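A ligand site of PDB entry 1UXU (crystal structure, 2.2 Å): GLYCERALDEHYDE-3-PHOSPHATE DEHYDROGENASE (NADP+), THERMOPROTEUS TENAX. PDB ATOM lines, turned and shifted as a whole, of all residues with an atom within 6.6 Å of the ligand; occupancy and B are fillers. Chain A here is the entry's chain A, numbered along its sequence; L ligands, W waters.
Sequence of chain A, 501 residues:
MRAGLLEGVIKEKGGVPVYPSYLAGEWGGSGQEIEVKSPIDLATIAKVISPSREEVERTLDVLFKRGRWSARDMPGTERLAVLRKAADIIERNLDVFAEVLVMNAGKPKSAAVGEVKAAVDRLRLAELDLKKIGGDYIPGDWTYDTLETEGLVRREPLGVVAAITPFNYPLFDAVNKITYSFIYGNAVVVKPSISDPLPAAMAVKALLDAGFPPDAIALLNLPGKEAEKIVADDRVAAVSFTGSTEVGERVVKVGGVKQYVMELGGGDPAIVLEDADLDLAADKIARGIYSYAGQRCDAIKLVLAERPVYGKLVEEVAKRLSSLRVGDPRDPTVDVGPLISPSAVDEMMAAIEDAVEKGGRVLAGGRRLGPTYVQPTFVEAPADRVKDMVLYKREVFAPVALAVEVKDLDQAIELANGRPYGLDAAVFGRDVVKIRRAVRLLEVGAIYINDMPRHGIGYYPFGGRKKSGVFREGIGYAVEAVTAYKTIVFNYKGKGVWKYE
Water W4 bridges O1 of the ligand (2.6 Å) and ND2 of Asn 168 (3.0 Å). Water W3 lies within hydrogen-bond range of O1 of the ligand (2.7 Å), OD2 of Asp 173 (2.9 Å) and ND2 of Asn 168 (3.3 Å). Water W6 bridges the backbone carbonyl oxygen of Gly 456 and an oxygen (O5) of the ligand. Water W1 bridges O2 of the ligand (3.2 Å) and SG of Cys 297 (3.7 Å). Water W7 lies within hydrogen-bond range of OD1 of Asp 173 (2.5 Å) and O2 of the ligand (3.3 Å).
The backbone NH (N) of His 455 sits at hydrogen-bond distance from an oxygen (O6) of the ligand, at 2.7 Å. A ring nitrogen (ND1) of His 455 lies within hydrogen-bond range of an oxygen (O2) of the ligand, 3.1 Å away. The side-chain amide nitrogen (ND2) of Asn 168 is in hydrogen-bond range of an oxygen (O1) of the ligand (2.9 Å). OD2 of Asp 298 lies close to O6 of the ligand. N of Gly 456 sits at hydrogen-bond distance from O5 of the ligand. NE of Arg 296 is in salt-bridge range of O4 of the ligand. The backbone NH (N) of Cys 297 lies close to an oxygen (O1) of the ligand, at 3.1 Å. The side-chain sulfur (SG) of Cys 297 is in hydrogen-bond range of an oxygen (O2) of the ligand. The side-chain hydroxyl (OH) of Tyr 169 sits at hydrogen-bond distance from an oxygen (O4) of the ligand (2.5 Å).
OD1 of Asp 298 lies within salt-bridge range of NH2 of Arg 296, 3.0 Å away. The backbone carbonyl oxygen (O) of Gln 295 lies close to the side-chain amide nitrogen (ND2) of Asn 168 (3.4 Å). NH2 of Arg 296 lies within hydrogen-bond range of O of Pro 453 (3.0 Å). OD2 of Asp 298 sits close to ND1 of His 455, 3.5 Å away. ND1 of His 455 sits close to SG of Cys 297 (3.7 Å).
Residues that only touch the ligand: Arg 454. The nearest printed residue that does not touch the ligand is Pro 453 (4.1 Å).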
ATOM      1  N   PRO A 166       6.251  -9.751  16.590  1.00  0.00           N
ATOM      2  CA  PRO A 166       5.784 -10.838  17.446  1.00  0.00           C
ATOM      3  C   PRO A 166       6.537 -12.148  17.104  1.00  0.00           C
ATOM      4  O   PRO A 166       7.327 -12.187  16.143  1.00  0.00           O
ATOM      5  CB  PRO A 166       4.319 -10.913  17.083  1.00  0.00           C
ATOM      6  CG  PRO A 166       4.389 -10.768  15.577  1.00  0.00           C
ATOM      7  CD  PRO A 166       5.455  -9.694  15.348  1.00  0.00           C
ATOM      8  N   ASN A 168       5.020 -15.210  16.233  1.00  0.00           N
ATOM      9  CA  ASN A 168       4.391 -16.101  15.277  1.00  0.00           C
ATOM     10  C   ASN A 168       4.719 -15.963  13.786  1.00  0.00           C
ATOM     11  O   ASN A 168       4.423 -16.878  13.006  1.00  0.00           O
ATOM     12  CB  ASN A 168       2.876 -16.109  15.516  1.00  0.00           C
ATOM     13  CG  ASN A 168       2.267 -14.732  15.492  1.00  0.00           C
ATOM     14  OD1 ASN A 168       2.753 -13.810  16.139  1.00  0.00           O
ATOM     15  ND2 ASN A 168       1.175 -14.588  14.752  1.00  0.00           N
ATOM     16  N   TYR A 169       5.296 -14.833  13.382  1.00  0.00           N
ATOM     17  CA  TYR A 169       5.715 -14.674  11.971  1.00  0.00           C
ATOM     18  C   TYR A 169       7.010 -13.893  12.032  1.00  0.00           C
ATOM     19  O   TYR A 169       7.109 -12.766  11.524  1.00  0.00           O
ATOM     20  CB  TYR A 169       4.679 -13.912  11.130  1.00  0.00           C
ATOM     21  CG  TYR A 169       3.496 -14.770  10.760  1.00  0.00           C
ATOM     22  CD1 TYR A 169       2.447 -14.951  11.643  1.00  0.00           C
ATOM     23  CD2 TYR A 169       3.460 -15.428   9.525  1.00  0.00           C
ATOM     24  CE1 TYR A 169       1.370 -15.781  11.321  1.00  0.00           C
ATOM     25  CE2 TYR A 169       2.391 -16.255   9.183  1.00  0.00           C
ATOM     26  CZ  TYR A 169       1.344 -16.421  10.093  1.00  0.00           C
ATOM     27  OH  TYR A 169       0.270 -17.238   9.789  1.00  0.00           O
ATOM     28  N   ASP A 173       6.683 -10.820   9.191  1.00  0.00           N
ATOM     29  CA  ASP A 173       6.421  -9.521   9.832  1.00  0.00           C
ATOM     30  C   ASP A 173       7.543  -8.516   9.745  1.00  0.00           C
ATOM     31  O   ASP A 173       7.301  -7.314   9.620  1.00  0.00           O
ATOM     32  CB  ASP A 173       6.029  -9.692  11.292  1.00  0.00           C
ATOM     33  CG  ASP A 173       4.591 -10.104  11.465  1.00  0.00           C
ATOM     34  OD1 ASP A 173       3.844 -10.070  10.445  1.00  0.00           O
ATOM     35  OD2 ASP A 173       4.205 -10.451  12.598  1.00  0.00           O
ATOM     36  N   THR A 242       2.837  -5.443  16.185  1.00  0.00           N
ATOM     37  CA  THR A 242       1.950  -6.588  16.070  1.00  0.00           C
ATOM     38  C   THR A 242       2.362  -7.360  17.301  1.00  0.00           C
ATOM     39  O   THR A 242       3.536  -7.736  17.447  1.00  0.00           O
ATOM     40  CB  THR A 242       2.181  -7.443  14.831  1.00  0.00           C
ATOM     41  OG1 THR A 242       1.895  -6.683  13.651  1.00  0.00           O
ATOM     42  CG2 THR A 242       1.231  -8.643  14.859  1.00  0.00           C
ATOM     43  N   GLU A 263      -1.694  -4.059  15.499  1.00  0.00           N
ATOM     44  CA  GLU A 263      -2.409  -5.272  15.102  1.00  0.00           C
ATOM     45  C   GLU A 263      -2.291  -6.074  16.386  1.00  0.00           C
ATOM     46  O   GLU A 263      -1.221  -6.651  16.678  1.00  0.00           O
ATOM     47  CB  GLU A 263      -1.687  -5.968  13.958  1.00  0.00           C
ATOM     48  CG  GLU A 263      -1.678  -5.200  12.679  1.00  0.00           C
ATOM     49  CD  GLU A 263      -2.967  -5.390  11.921  1.00  0.00           C
ATOM     50  OE1 GLU A 263      -3.765  -6.270  12.341  1.00  0.00           O
ATOM     51  OE2 GLU A 263      -3.187  -4.680  10.900  1.00  0.00           O
ATOM     52  N   GLY A 265      -4.382  -8.673  17.392  1.00  0.00           N
ATOM     53  CA  GLY A 265      -5.001  -9.983  17.380  1.00  0.00           C
ATOM     54  C   GLY A 265      -6.251 -10.246  18.227  1.00  0.00           C
ATOM     55  O   GLY A 265      -7.200  -9.459  18.217  1.00  0.00           O
ATOM     56  N   SER A 291      -4.316 -24.214  12.397  1.00  0.00           N
ATOM     57  CA  SER A 291      -3.097 -23.730  11.735  1.00  0.00           C
ATOM     58  C   SER A 291      -2.082 -23.141  12.680  1.00  0.00           C
ATOM     59  O   SER A 291      -2.407 -22.272  13.505  1.00  0.00           O
ATOM     60  CB  SER A 291      -3.402 -22.722  10.651  1.00  0.00           C
ATOM     61  OG  SER A 291      -4.059 -23.368   9.581  1.00  0.00           O
ATOM     62  N   GLN A 295      -1.662 -20.460  16.754  1.00  0.00           N
ATOM     63  CA  GLN A 295      -0.865 -19.281  17.098  1.00  0.00           C
ATOM     64  C   GLN A 295      -0.891 -18.210  16.003  1.00  0.00           C
ATOM     65  O   GLN A 295       0.145 -17.727  15.547  1.00  0.00           O
ATOM     66  CB  GLN A 295       0.562 -19.691  17.445  1.00  0.00           C
ATOM     67  CG  GLN A 295       0.655 -20.514  18.721  1.00  0.00           C
ATOM     68  CD  GLN A 295       2.015 -21.151  18.933  1.00  0.00           C
ATOM     69  OE1 GLN A 295       2.551 -21.121  20.032  1.00  0.00           O
ATOM     70  NE2 GLN A 295       2.583 -21.727  17.861  1.00  0.00           N
ATOM     71  N   ARG A 296      -2.111 -17.855  15.606  1.00  0.00           N
ATOM     72  CA  ARG A 296      -2.349 -16.850  14.584  1.00  0.00           C
ATOM     73  C   ARG A 296      -3.333 -15.788  15.120  1.00  0.00           C
ATOM     74  O   ARG A 296      -4.381 -16.127  15.692  1.00  0.00           O
ATOM     75  CB  ARG A 296      -2.950 -17.481  13.339  1.00  0.00           C
ATOM     76  CG  ARG A 296      -2.004 -18.350  12.566  1.00  0.00           C
ATOM     77  CD  ARG A 296      -2.777 -19.175  11.572  1.00  0.00           C
ATOM     78  NE  ARG A 296      -3.350 -18.350  10.514  1.00  0.00           N
ATOM     79  CZ  ARG A 296      -4.636 -18.352  10.196  1.00  0.00           C
ATOM     80  NH1 ARG A 296      -5.498 -19.110  10.877  1.00  0.00           N
ATOM     81  NH2 ARG A 296      -5.060 -17.624   9.173  1.00  0.00           N
ATOM     82  N   CYS A 297      -2.976 -14.526  14.933  1.00  0.00           N
ATOM     83  CA  CYS A 297      -3.815 -13.414  15.371  1.00  0.00           C
ATOM     84  C   CYS A 297      -5.260 -13.669  14.945  1.00  0.00           C
ATOM     85  O   CYS A 297      -6.178 -13.375  15.693  1.00  0.00           O
ATOM     86  CB  CYS A 297      -3.338 -12.105  14.737  1.00  0.00           C
ATOM     87  SG  CYS A 297      -3.523 -12.193  12.958  1.00  0.00           S
ATOM     88  N   ASP A 298      -5.449 -14.252  13.753  1.00  0.00           N
ATOM     89  CA  ASP A 298      -6.772 -14.551  13.251  1.00  0.00           C
ATOM     90  C   ASP A 298      -7.250 -16.014  13.362  1.00  0.00           C
ATOM     91  O   ASP A 298      -8.044 -16.483  12.549  1.00  0.00           O
ATOM     92  CB  ASP A 298      -6.907 -14.086  11.786  1.00  0.00           C
ATOM     93  CG  ASP A 298      -5.818 -14.644  10.872  1.00  0.00           C
ATOM     94  OD1 ASP A 298      -5.044 -15.556  11.291  1.00  0.00           O
ATOM     95  OD2 ASP A 298      -5.730 -14.171   9.717  1.00  0.00           O
ATOM     96  N   PHE A 397      -4.032 -18.246  23.325  1.00  0.00           N
ATOM     97  CA  PHE A 397      -3.189 -18.454  22.146  1.00  0.00           C
ATOM     98  C   PHE A 397      -2.750 -19.920  22.067  1.00  0.00           C
ATOM     99  O   PHE A 397      -1.716 -20.313  22.596  1.00  0.00           O
ATOM    100  CB  PHE A 397      -1.983 -17.495  22.167  1.00  0.00           C
ATOM    101  CG  PHE A 397      -1.655 -16.924  20.807  1.00  0.00           C
ATOM    102  CD1 PHE A 397      -2.673 -16.389  20.000  1.00  0.00           C
ATOM    103  CD2 PHE A 397      -0.362 -16.955  20.308  1.00  0.00           C
ATOM    104  CE1 PHE A 397      -2.389 -15.900  18.709  1.00  0.00           C
ATOM    105  CE2 PHE A 397      -0.065 -16.464  19.019  1.00  0.00           C
ATOM    106  CZ  PHE A 397      -1.081 -15.939  18.225  1.00  0.00           C
ATOM    107  N   LEU A 423     -11.023  -8.423  15.306  1.00  0.00           N
ATOM    108  CA  LEU A 423     -10.067  -8.477  14.193  1.00  0.00           C
ATOM    109  C   LEU A 423     -10.790  -8.855  12.904  1.00  0.00           C
ATOM    110  O   LEU A 423     -10.983  -7.997  12.044  1.00  0.00           O
ATOM    111  CB  LEU A 423      -8.952  -9.473  14.482  1.00  0.00           C
ATOM    112  CG  LEU A 423      -7.767  -9.413  13.504  1.00  0.00           C
ATOM    113  CD1 LEU A 423      -7.116  -8.005  13.556  1.00  0.00           C
ATOM    114  CD2 LEU A 423      -6.724 -10.503  13.883  1.00  0.00           C
ATOM    115  N   TYR A 448     -14.728 -12.343   6.387  1.00  0.00           N
ATOM    116  CA  TYR A 448     -14.435 -13.271   5.302  1.00  0.00           C
ATOM    117  C   TYR A 448     -15.691 -14.051   4.974  1.00  0.00           C
ATOM    118  O   TYR A 448     -16.189 -14.786   5.801  1.00  0.00           O
ATOM    119  CB  TYR A 448     -13.287 -14.212   5.685  1.00  0.00           C
ATOM    120  CG  TYR A 448     -11.958 -13.499   5.727  1.00  0.00           C
ATOM    121  CD1 TYR A 448     -11.602 -12.741   6.831  1.00  0.00           C
ATOM    122  CD2 TYR A 448     -11.094 -13.507   4.610  1.00  0.00           C
ATOM    123  CE1 TYR A 448     -10.414 -11.985   6.853  1.00  0.00           C
ATOM    124  CE2 TYR A 448      -9.911 -12.764   4.615  1.00  0.00           C
ATOM    125  CZ  TYR A 448      -9.579 -11.998   5.734  1.00  0.00           C
ATOM    126  OH  TYR A 448      -8.444 -11.227   5.755  1.00  0.00           O
ATOM    127  N   MET A 452     -12.013 -19.117   5.519  1.00  0.00           N
ATOM    128  CA  MET A 452     -11.442 -18.836   6.826  1.00  0.00           C
ATOM    129  C   MET A 452     -10.675 -17.521   6.710  1.00  0.00           C
ATOM    130  O   MET A 452     -10.199 -17.145   5.634  1.00  0.00           O
ATOM    131  CB  MET A 452     -10.474 -19.955   7.286  1.00  0.00           C
ATOM    132  CG  MET A 452      -9.216 -20.150   6.420  1.00  0.00           C
ATOM    133  SD  MET A 452      -7.938 -21.227   7.193  1.00  0.00           S
ATOM    134  CE  MET A 452      -6.961 -20.064   8.037  1.00  0.00           C
ATOM    135  N   PRO A 453     -10.559 -16.793   7.821  1.00  0.00           N
ATOM    136  CA  PRO A 453      -9.840 -15.531   7.777  1.00  0.00           C
ATOM    137  C   PRO A 453      -8.360 -15.834   7.504  1.00  0.00           C
ATOM    138  O   PRO A 453      -7.755 -16.625   8.233  1.00  0.00           O
ATOM    139  CB  PRO A 453     -10.028 -14.962   9.184  1.00  0.00           C
ATOM    140  CG  PRO A 453     -11.297 -15.609   9.644  1.00  0.00           C
ATOM    141  CD  PRO A 453     -11.189 -17.010   9.126  1.00  0.00           C
ATOM    142  N   ARG A 454      -7.794 -15.186   6.479  1.00  0.00           N
ATOM    143  CA  ARG A 454      -6.377 -15.374   6.145  1.00  0.00           C
ATOM    144  C   ARG A 454      -5.782 -14.069   5.570  1.00  0.00           C
ATOM    145  O   ARG A 454      -6.185 -13.585   4.493  1.00  0.00           O
ATOM    146  CB  ARG A 454      -6.190 -16.547   5.156  1.00  0.00           C
ATOM    147  CG  ARG A 454      -4.755 -17.135   5.249  1.00  0.00           C
ATOM    148  CD  ARG A 454      -4.510 -18.373   4.370  1.00  0.00           C
ATOM    149  NE  ARG A 454      -4.105 -18.016   3.006  1.00  0.00           N
ATOM    150  CZ  ARG A 454      -4.958 -17.821   2.002  1.00  0.00           C
ATOM    151  NH1 ARG A 454      -6.288 -17.940   2.213  1.00  0.00           N
ATOM    152  NH2 ARG A 454      -4.491 -17.497   0.802  1.00  0.00           N
ATOM    153  N   HIS A 455      -4.830 -13.506   6.305  1.00  0.00           N
ATOM    154  CA  HIS A 455      -4.214 -12.254   5.894  1.00  0.00           C
ATOM    155  C   HIS A 455      -3.240 -12.383   4.721  1.00  0.00           C
ATOM    156  O   HIS A 455      -3.138 -11.466   3.905  1.00  0.00           O
ATOM    157  CB  HIS A 455      -3.582 -11.624   7.122  1.00  0.00           C
ATOM    158  CG  HIS A 455      -4.594 -11.230   8.175  1.00  0.00           C
ATOM    159  ND1 HIS A 455      -4.261 -11.043   9.496  1.00  0.00           N
ATOM    160  CD2 HIS A 455      -5.931 -11.039   8.079  1.00  0.00           C
ATOM    161  CE1 HIS A 455      -5.359 -10.761  10.182  1.00  0.00           C
ATOM    162  NE2 HIS A 455      -6.384 -10.760   9.354  1.00  0.00           N
ATOM    163  N   GLY A 456      -2.548 -13.516   4.604  1.00  0.00           N
ATOM    164  CA  GLY A 456      -1.617 -13.690   3.500  1.00  0.00           C
ATOM    165  C   GLY A 456      -0.602 -12.570   3.451  1.00  0.00           C
ATOM    166  O   GLY A 456      -0.070 -12.165   4.487  1.00  0.00           O
ATOM    167  N   ILE A 457      -0.320 -12.047   2.276  1.00  0.00           N
ATOM    168  CA  ILE A 457       0.649 -10.957   2.219  1.00  0.00           C
ATOM    169  C   ILE A 457       0.018  -9.573   2.431  1.00  0.00           C
ATOM    170  O   ILE A 457       0.699  -8.555   2.355  1.00  0.00           O
ATOM    171  CB  ILE A 457       1.392 -10.964   0.855  1.00  0.00           C
ATOM    172  CG1 ILE A 457       0.431 -10.656  -0.269  1.00  0.00           C
ATOM    173  CG2 ILE A 457       2.067 -12.337   0.614  1.00  0.00           C
ATOM    174  CD1 ILE A 457       1.121 -10.368  -1.565  1.00  0.00           C
ATOM    175  N   PHE A 462      -6.247  -5.246   6.525  1.00  0.00           N
ATOM    176  CA  PHE A 462      -6.832  -5.894   7.684  1.00  0.00           C
ATOM    177  C   PHE A 462      -6.280  -5.225   8.932  1.00  0.00           C
ATOM    178  O   PHE A 462      -5.186  -4.663   8.891  1.00  0.00           O
ATOM    179  CB  PHE A 462      -6.463  -7.381   7.695  1.00  0.00           C
ATOM    180  CG  PHE A 462      -4.981  -7.631   7.879  1.00  0.00           C
ATOM    181  CD1 PHE A 462      -4.142  -7.722   6.771  1.00  0.00           C
ATOM    182  CD2 PHE A 462      -4.425  -7.740   9.155  1.00  0.00           C
ATOM    183  CE1 PHE A 462      -2.752  -7.918   6.927  1.00  0.00           C
ATOM    184  CE2 PHE A 462      -3.039  -7.931   9.331  1.00  0.00           C
ATOM    185  CZ  PHE A 462      -2.205  -8.019   8.211  1.00  0.00           C
ATOM    186  N   GLU A 473      -2.842  -2.802   8.019  1.00  0.00           N
ATOM    187  CA  GLU A 473      -1.633  -3.175   7.300  1.00  0.00           C
ATOM    188  C   GLU A 473      -2.237  -3.661   5.994  1.00  0.00           C
ATOM    189  O   GLU A 473      -3.451  -3.894   5.917  1.00  0.00           O
ATOM    190  CB  GLU A 473      -0.844  -4.296   7.988  1.00  0.00           C
ATOM    191  CG  GLU A 473      -0.058  -3.816   9.195  1.00  0.00           C
ATOM    192  CD  GLU A 473       0.969  -4.834   9.698  1.00  0.00           C
ATOM    193  OE1 GLU A 473       0.610  -6.033   9.794  1.00  0.00           O
ATOM    194  OE2 GLU A 473       2.123  -4.437  10.004  1.00  0.00           O
HETATM  195  O1  LIG L   1      -0.745 -12.822  13.525  1.00  0.00           O
HETATM  196  C1  LIG L   1      -1.096 -13.539  12.609  1.00  0.00           C
HETATM  197  C2  LIG L   1      -0.889 -13.137  11.134  1.00  0.00           C
HETATM  198  O2  LIG L   1      -1.702 -11.976  10.871  1.00  0.00           O
HETATM  199  C3  LIG L   1      -1.234 -14.365  10.319  1.00  0.00           C
HETATM  200  O3  LIG L   1      -1.922 -14.183   9.099  1.00  0.00           O
HETATM  201  O4  LIG L   1      -1.956 -16.656   8.765  1.00  0.00           O
HETATM  202  O5  LIG L   1      -1.690 -15.089   6.828  1.00  0.00           O
HETATM  203  O6  LIG L   1      -3.880 -15.287   8.035  1.00  0.00           O
HETATM  204  P1  LIG L   1      -2.384 -15.387   8.116  1.00  0.00           P
HETATM  205  O   HOH W   1      -1.469  -9.196  12.538  1.00  0.00           O
HETATM  206  O   HOH W   2       0.315 -11.054   8.416  1.00  0.00           O
HETATM  207  O   HOH W   3       1.672 -11.729  13.189  1.00  0.00           O
HETATM  208  O   HOH W   4       0.059 -12.095  15.941  1.00  0.00           O
HETATM  209  O   HOH W   5      -0.424 -17.042   4.557  1.00  0.00           O
HETATM  210  O   HOH W   6       0.497 -13.213   6.883  1.00  0.00           O
HETATM  211  O   HOH W   7       1.448 -10.856  10.730  1.00  0.00           O
